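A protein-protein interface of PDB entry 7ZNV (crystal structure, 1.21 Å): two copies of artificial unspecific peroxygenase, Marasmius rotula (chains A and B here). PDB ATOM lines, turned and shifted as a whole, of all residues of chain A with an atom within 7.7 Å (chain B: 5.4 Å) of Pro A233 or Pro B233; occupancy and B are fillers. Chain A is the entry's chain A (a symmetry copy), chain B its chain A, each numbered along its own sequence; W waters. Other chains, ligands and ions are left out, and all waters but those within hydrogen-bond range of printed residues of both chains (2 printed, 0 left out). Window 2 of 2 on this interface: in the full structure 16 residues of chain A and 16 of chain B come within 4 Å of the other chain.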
ATOM      1  N   GLY A  89      14.308 -29.204  29.155  1.00  0.00           N
ATOM      2  CA  GLY A  89      13.275 -28.312  28.644  1.00  0.00           C
ATOM      3  C   GLY A  89      13.571 -26.853  28.849  1.00  0.00           C
ATOM      4  O   GLY A  89      12.807 -26.017  28.368  1.00  0.00           O
ATOM      5  N   THR A 152      10.387 -33.844  22.427  1.00  0.00           N
ATOM      6  CA  THR A 152       9.973 -32.468  22.273  1.00  0.00           C
ATOM      7  C   THR A 152      10.809 -31.890  21.141  1.00  0.00           C
ATOM      8  O   THR A 152      12.077 -31.869  21.242  1.00  0.00           O
ATOM      9  CB  THR A 152      10.126 -31.671  23.564  1.00  0.00           C
ATOM     10  OG1 THR A 152       9.355 -32.319  24.583  1.00  0.00           O
ATOM     11  CG2 THR A 152       9.619 -30.265  23.365  1.00  0.00           C
ATOM     12  N   ASN A 153      10.175 -31.498  20.071  1.00  0.00           N
ATOM     13  CA  ASN A 153      10.814 -31.088  18.815  1.00  0.00           C
ATOM     14  C   ASN A 153      10.072 -29.896  18.244  1.00  0.00           C
ATOM     15  O   ASN A 153       9.199 -30.059  17.384  1.00  0.00           O
ATOM     16  CB  ASN A 153      10.843 -32.239  17.839  1.00  0.00           C
ATOM     17  CG  ASN A 153      11.289 -31.796  16.466  1.00  0.00           C
ATOM     18  OD1 ASN A 153      12.237 -31.007  16.331  1.00  0.00           O
ATOM     19  ND2 ASN A 153      10.633 -32.302  15.438  1.00  0.00           N
ATOM     20  N   THR A 154      10.342 -28.741  18.760  1.00  0.00           N
ATOM     21  CA  THR A 154       9.766 -27.477  18.266  1.00  0.00           C
ATOM     22  C   THR A 154      10.853 -26.639  17.612  1.00  0.00           C
ATOM     23  O   THR A 154      12.051 -26.980  17.682  1.00  0.00           O
ATOM     24  CB  THR A 154       9.074 -26.675  19.363  1.00  0.00           C
ATOM     25  OG1 THR A 154       9.993 -25.908  20.133  1.00  0.00           O
ATOM     26  CG2 THR A 154       8.217 -27.524  20.287  1.00  0.00           C
ATOM     27  N   GLY A 155      10.477 -25.516  17.053  1.00  0.00           N
ATOM     28  CA  GLY A 155      11.460 -24.566  16.537  1.00  0.00           C
ATOM     29  C   GLY A 155      12.445 -24.119  17.594  1.00  0.00           C
ATOM     30  O   GLY A 155      13.583 -23.762  17.224  1.00  0.00           O
ATOM     31  N   LYS A 156      12.111 -24.119  18.869  1.00  0.00           N
ATOM     32  CA  LYS A 156      13.059 -23.741  19.909  1.00  0.00           C
ATOM     33  C   LYS A 156      14.205 -24.749  19.938  1.00  0.00           C
ATOM     34  O   LYS A 156      15.381 -24.350  19.849  1.00  0.00           O
ATOM     35  CB  LYS A 156      12.383 -23.642  21.257  1.00  0.00           C
ATOM     36  CG  LYS A 156      13.368 -23.210  22.322  1.00  0.00           C
ATOM     37  CD  LYS A 156      13.105 -23.490  23.755  1.00  0.00           C
ATOM     38  CE  LYS A 156      13.690 -24.755  24.252  1.00  0.00           C
ATOM     39  NZ  LYS A 156      13.450 -25.011  25.687  1.00  0.00           N
ATOM     40  N   GLU A 157      13.883 -26.009  20.113  1.00  0.00           N
ATOM     41  CA  GLU A 157      14.925 -27.037  20.179  1.00  0.00           C
ATOM     42  C   GLU A 157      15.683 -27.101  18.892  1.00  0.00           C
ATOM     43  O   GLU A 157      16.947 -27.278  18.946  1.00  0.00           O
ATOM     44  CB  GLU A 157      14.364 -28.415  20.503  1.00  0.00           C
ATOM     45  CG  GLU A 157      13.736 -28.505  21.884  1.00  0.00           C
ATOM     46  CD  GLU A 157      12.357 -27.910  22.041  1.00  0.00           C
ATOM     47  OE1 GLU A 157      11.710 -27.688  21.051  1.00  0.00           O
ATOM     48  OE2 GLU A 157      11.986 -27.722  23.224  1.00  0.00           O
ATOM     49  N   ASN A 228       7.317 -30.878  15.379  1.00  0.00           N
ATOM     50  CA  ASN A 228       6.075 -31.596  15.791  1.00  0.00           C
ATOM     51  C   ASN A 228       4.972 -30.477  15.768  1.00  0.00           C
ATOM     52  O   ASN A 228       5.020 -29.388  16.414  1.00  0.00           O
ATOM     53  CB  ASN A 228       6.241 -32.219  17.174  1.00  0.00           C
ATOM     54  CG  ASN A 228       4.950 -32.771  17.742  1.00  0.00           C
ATOM     55  OD1 ASN A 228       3.869 -32.226  17.519  1.00  0.00           O
ATOM     56  ND2 ASN A 228       5.051 -33.854  18.493  1.00  0.00           N
ATOM     57  N   ASP A 230       2.025 -30.110  16.943  1.00  0.00           N
ATOM     58  CA  ASP A 230       1.115 -29.999  18.115  1.00  0.00           C
ATOM     59  C   ASP A 230       1.844 -29.457  19.348  1.00  0.00           C
ATOM     60  O   ASP A 230       1.228 -29.434  20.403  1.00  0.00           O
ATOM     61  CB  ASP A 230       0.508 -31.367  18.443  1.00  0.00           C
ATOM     62  CG  ASP A 230      -0.339 -31.891  17.287  1.00  0.00           C
ATOM     63  OD1 ASP A 230      -1.000 -31.051  16.621  1.00  0.00           O
ATOM     64  OD2 ASP A 230      -0.274 -33.108  17.019  1.00  0.00           O
ATOM     65  N   GLN A 231       3.128 -29.089  19.258  1.00  0.00           N
ATOM     66  CA  GLN A 231       3.912 -28.713  20.455  1.00  0.00           C
ATOM     67  C   GLN A 231       4.237 -27.221  20.421  1.00  0.00           C
ATOM     68  O   GLN A 231       4.740 -26.670  19.451  1.00  0.00           O
ATOM     69  CB  GLN A 231       5.206 -29.513  20.488  1.00  0.00           C
ATOM     70  CG  GLN A 231       4.975 -30.985  20.782  1.00  0.00           C
ATOM     71  CD  GLN A 231       6.269 -31.761  20.788  1.00  0.00           C
ATOM     72  OE1 GLN A 231       7.324 -31.322  20.296  1.00  0.00           O
ATOM     73  NE2 GLN A 231       6.222 -32.898  21.427  1.00  0.00           N
ATOM     74  N   CYS A 232       3.877 -26.498  21.478  1.00  0.00           N
ATOM     75  CA  CYS A 232       4.259 -25.084  21.645  1.00  0.00           C
ATOM     76  C   CYS A 232       5.672 -25.007  22.207  1.00  0.00           C
ATOM     77  O   CYS A 232       5.958 -25.668  23.226  1.00  0.00           O
ATOM     78  CB  CYS A 232       3.340 -24.346  22.599  1.00  0.00           C
ATOM     79  SG  CYS A 232       1.646 -24.067  22.073  1.00  0.00           S
ATOM     80  N   PRO A 233       6.537 -24.184  21.622  1.00  0.00           N
ATOM     81  CA  PRO A 233       7.875 -24.020  22.188  1.00  0.00           C
ATOM     82  C   PRO A 233       7.769 -23.480  23.604  1.00  0.00           C
ATOM     83  O   PRO A 233       6.922 -22.567  23.883  1.00  0.00           O
ATOM     84  CB  PRO A 233       8.519 -23.025  21.254  1.00  0.00           C
ATOM     85  CG  PRO A 233       7.741 -23.059  19.966  1.00  0.00           C
ATOM     86  CD  PRO A 233       6.317 -23.388  20.411  1.00  0.00           C
ATOM     87  N   TRP A 234       8.683 -23.851  24.486  1.00  0.00           N
ATOM     88  CA  TRP A 234       8.628 -23.334  25.870  1.00  0.00           C
ATOM     89  C   TRP A 234       9.997 -23.454  26.494  1.00  0.00           C
ATOM     90  O   TRP A 234      10.758 -24.384  26.164  1.00  0.00           O
ATOM     91  CB  TRP A 234       7.570 -24.090  26.684  1.00  0.00           C
ATOM     92  CG  TRP A 234       7.338 -23.518  28.051  1.00  0.00           C
ATOM     93  CD1 TRP A 234       7.625 -24.110  29.232  1.00  0.00           C
ATOM     94  CD2 TRP A 234       6.788 -22.223  28.371  1.00  0.00           C
ATOM     95  NE1 TRP A 234       7.322 -23.250  30.262  1.00  0.00           N
ATOM     96  CE2 TRP A 234       6.864 -22.079  29.769  1.00  0.00           C
ATOM     97  CE3 TRP A 234       6.352 -21.148  27.598  1.00  0.00           C
ATOM     98  CZ2 TRP A 234       6.354 -20.947  30.412  1.00  0.00           C
ATOM     99  CZ3 TRP A 234       5.934 -19.984  28.229  1.00  0.00           C
ATOM    100  CH2 TRP A 234       5.933 -19.911  29.623  1.00  0.00           C
ATOM    101  N   ILE A 235      10.292 -22.550  27.392  1.00  0.00           N
ATOM    102  CA  ILE A 235      11.457 -22.649  28.289  1.00  0.00           C
ATOM    103  C   ILE A 235      10.983 -23.017  29.673  1.00  0.00           C
ATOM    104  O   ILE A 235      10.332 -22.173  30.330  1.00  0.00           O
ATOM    105  CB  ILE A 235      12.249 -21.348  28.254  1.00  0.00           C
ATOM    106  CG1 ILE A 235      12.782 -21.070  26.857  1.00  0.00           C
ATOM    107  CG2 ILE A 235      13.379 -21.420  29.265  1.00  0.00           C
ATOM    108  CD1 ILE A 235      13.417 -19.709  26.671  1.00  0.00           C
ATOM    109  N   VAL A 236      11.307 -24.203  30.160  1.00  0.00           N
ATOM    110  CA  VAL A 236      10.976 -24.580  31.547  1.00  0.00           C
ATOM    111  C   VAL A 236      11.602 -23.579  32.495  1.00  0.00           C
ATOM    112  O   VAL A 236      12.820 -23.279  32.411  1.00  0.00           O
ATOM    113  CB  VAL A 236      11.417 -26.026  31.807  1.00  0.00           C
ATOM    114  CG1 VAL A 236      11.354 -26.377  33.278  1.00  0.00           C
ATOM    115  CG2 VAL A 236      10.583 -26.998  30.992  1.00  0.00           C
ATOM    116  N   THR B 154      -2.773 -15.750  26.856  1.00  0.00           N
ATOM    117  CA  THR B 154      -2.487 -17.171  27.129  1.00  0.00           C
ATOM    118  C   THR B 154      -2.457 -17.408  28.630  1.00  0.00           C
ATOM    119  O   THR B 154      -2.508 -16.451  29.429  1.00  0.00           O
ATOM    120  CB  THR B 154      -1.184 -17.644  26.496  1.00  0.00           C
ATOM    121  OG1 THR B 154      -0.047 -17.307  27.284  1.00  0.00           O
ATOM    122  CG2 THR B 154      -0.985 -17.148  25.073  1.00  0.00           C
ATOM    123  N   GLY B 155      -2.292 -18.645  29.030  1.00  0.00           N
ATOM    124  CA  GLY B 155      -2.091 -18.960  30.442  1.00  0.00           C
ATOM    125  C   GLY B 155      -0.902 -18.237  31.034  1.00  0.00           C
ATOM    126  O   GLY B 155      -0.913 -17.989  32.258  1.00  0.00           O
ATOM    127  N   LYS B 156       0.111 -17.872  30.274  1.00  0.00           N
ATOM    128  CA  LYS B 156       1.245 -17.132  30.812  1.00  0.00           C
ATOM    129  C   LYS B 156       0.773 -15.763  31.292  1.00  0.00           C
ATOM    130  O   LYS B 156       1.016 -15.399  32.458  1.00  0.00           O
ATOM    131  CB  LYS B 156       2.350 -17.001  29.788  1.00  0.00           C
ATOM    132  CG  LYS B 156       3.538 -16.266  30.370  1.00  0.00           C
ATOM    133  CD  LYS B 156       4.524 -15.598  29.484  1.00  0.00           C
ATOM    134  CE  LYS B 156       4.241 -14.171  29.217  1.00  0.00           C
ATOM    135  NZ  LYS B 156       5.243 -13.505  28.360  1.00  0.00           N
ATOM    136  N   GLN B 231      -3.098 -19.453  20.643  1.00  0.00           N
ATOM    137  CA  GLN B 231      -1.850 -18.737  20.987  1.00  0.00           C
ATOM    138  C   GLN B 231      -0.993 -19.594  21.916  1.00  0.00           C
ATOM    139  O   GLN B 231      -1.427 -20.108  22.938  1.00  0.00           O
ATOM    140  CB  GLN B 231      -2.189 -17.424  21.677  1.00  0.00           C
ATOM    141  CG  GLN B 231      -2.816 -16.413  20.734  1.00  0.00           C
ATOM    142  CD  GLN B 231      -3.163 -15.129  21.444  1.00  0.00           C
ATOM    143  OE1 GLN B 231      -3.233 -15.039  22.683  1.00  0.00           O
ATOM    144  NE2 GLN B 231      -3.303 -14.092  20.664  1.00  0.00           N
ATOM    145  N   CYS B 232       0.258 -19.839  21.534  1.00  0.00           N
ATOM    146  CA  CYS B 232       1.237 -20.521  22.399  1.00  0.00           C
ATOM    147  C   CYS B 232       1.842 -19.514  23.368  1.00  0.00           C
ATOM    148  O   CYS B 232       2.311 -18.448  22.921  1.00  0.00           O
ATOM    149  CB  CYS B 232       2.371 -21.144  21.609  1.00  0.00           C
ATOM    150  SG  CYS B 232       1.979 -22.543  20.553  1.00  0.00           S
ATOM    151  N   PRO B 233       1.905 -19.839  24.654  1.00  0.00           N
ATOM    152  CA  PRO B 233       2.557 -18.933  25.599  1.00  0.00           C
ATOM    153  C   PRO B 233       4.014 -18.749  25.205  1.00  0.00           C
ATOM    154  O   PRO B 233       4.704 -19.745  24.808  1.00  0.00           O
ATOM    155  CB  PRO B 233       2.419 -19.657  26.915  1.00  0.00           C
ATOM    156  CG  PRO B 233       1.294 -20.645  26.761  1.00  0.00           C
ATOM    157  CD  PRO B 233       1.362 -21.045  25.288  1.00  0.00           C
ATOM    158  N   TRP B 234       4.584 -17.580  25.449  1.00  0.00           N
ATOM    159  CA  TRP B 234       6.004 -17.363  25.099  1.00  0.00           C
ATOM    160  C   TRP B 234       6.543 -16.218  25.922  1.00  0.00           C
ATOM    161  O   TRP B 234       5.795 -15.282  26.261  1.00  0.00           O
ATOM    162  CB  TRP B 234       6.153 -17.096  23.597  1.00  0.00           C
ATOM    163  CG  TRP B 234       7.578 -17.027  23.134  1.00  0.00           C
ATOM    164  CD1 TRP B 234       8.219 -15.936  22.655  1.00  0.00           C
ATOM    165  CD2 TRP B 234       8.544 -18.098  23.129  1.00  0.00           C
ATOM    166  NE1 TRP B 234       9.531 -16.254  22.390  1.00  0.00           N
ATOM    167  CE2 TRP B 234       9.771 -17.542  22.718  1.00  0.00           C
ATOM    168  CE3 TRP B 234       8.504 -19.429  23.541  1.00  0.00           C
ATOM    169  CZ2 TRP B 234      10.909 -18.336  22.551  1.00  0.00           C
ATOM    170  CZ3 TRP B 234       9.658 -20.198  23.467  1.00  0.00           C
ATOM    171  CH2 TRP B 234      10.834 -19.640  22.964  1.00  0.00           C
ATOM    172  N   ILE B 235       7.817 -16.280  26.213  1.00  0.00           N
ATOM    173  CA  ILE B 235       8.576 -15.148  26.773  1.00  0.00           C
ATOM    174  C   ILE B 235       9.455 -14.561  25.697  1.00  0.00           C
ATOM    175  O   ILE B 235      10.428 -15.232  25.284  1.00  0.00           O
ATOM    176  CB  ILE B 235       9.356 -15.603  28.000  1.00  0.00           C
ATOM    177  CG1 ILE B 235       8.419 -16.100  29.090  1.00  0.00           C
ATOM    178  CG2 ILE B 235      10.220 -14.460  28.501  1.00  0.00           C
ATOM    179  CD1 ILE B 235       9.100 -16.754  30.273  1.00  0.00           C
HETATM  180  O   HOH W   1       4.373 -22.350  24.774  1.00  0.00           O
HETATM  181  O   HOH W   2       5.367 -20.974  22.488  1.00  0.00           O
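Of the 15 printed residues of chain A, 3 touch a printed residue of chain B.
Hydrophobic or aromatic side chains of chain A that line the printed part of chain B: Pro A233 and Trp A234.
Hydrophobic or aromatic side chains of chain B within 4 Å of the printed part of chain A: Pro B233 and Trp B234.
Along chain B the printed residues that touch a printed residue of chain A span positions 232 to 234.
Among the printed residues, no Asp or Glu carboxylate lies within 4 Å of a Lys or Arg side-chain nitrogen of the other chain.
Asn A153 touches none of the printed residues of chain B.
Asp A230 touches none of the printed residues of chain B.
Of the printed residues of chain B, Cys A232 touches Cys B232.
Pro A233 touches two residues of chain B.
Printed residues of chain B within 4 Å of Trp A234: Pro B233 (3.5 Å) and Trp B234 (3.9 Å).
Of the printed residues of chain A, Cys B232 touches Cys A232.
Of chain A, only Pro A233 (3.7 Å) and Trp A234 (3.5 Å) come within 4 Å of Pro B233.
Of the printed residues of chain A, Trp B234 touches Pro A233 (3.5 Å) and Trp A234 (3.9 Å).
The nearest residue of chain B that does not touch Pro A233 is Cys B232 (4.4 Å).
SG of Cys B232 forms a disulfide with SG of Cys A232, at 2.2 Å.
Cys B232 touches its own counterpart, Cys A232.
Pro B233 touches its own counterpart, Pro A233.
Pro A233 touches Trp B234, and with the chains exchanged Trp A234 touches Pro B233.
Trp A234 touches its own counterpart, Trp B234.
Of the 5 pairs that touch across the chains among the printed residues, 5 have their exchanged pair printed and touching as well.
Water W2 bridges the backbone carbonyl oxygen of Pro A233 and the backbone carbonyl oxygen of Pro B233.
Water W1 lies within hydrogen-bond range of O of Pro B233 (2.6 Å) and O of Pro A233 (2.7 Å).
The side-chain amino group of Lys B156 sits at hydrogen-bond distance from the backbone carbonyl oxygen of Trp B234 (2.8 Å).
The backbone carbonyl oxygen (O) of Trp A234 is in hydrogen-bond range of the side-chain amino group (NZ) of Lys A156, at 2.8 Å.
O of Pro A233 touches O of Pro B233, 3.7 Å away.
Trp B234 touches Pro A233.
Pro B233 touches Trp A234 (O to CE3, 3.5 Å).
CZ3 of Trp A234 touches N of Trp B234, at 3.9 Å.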
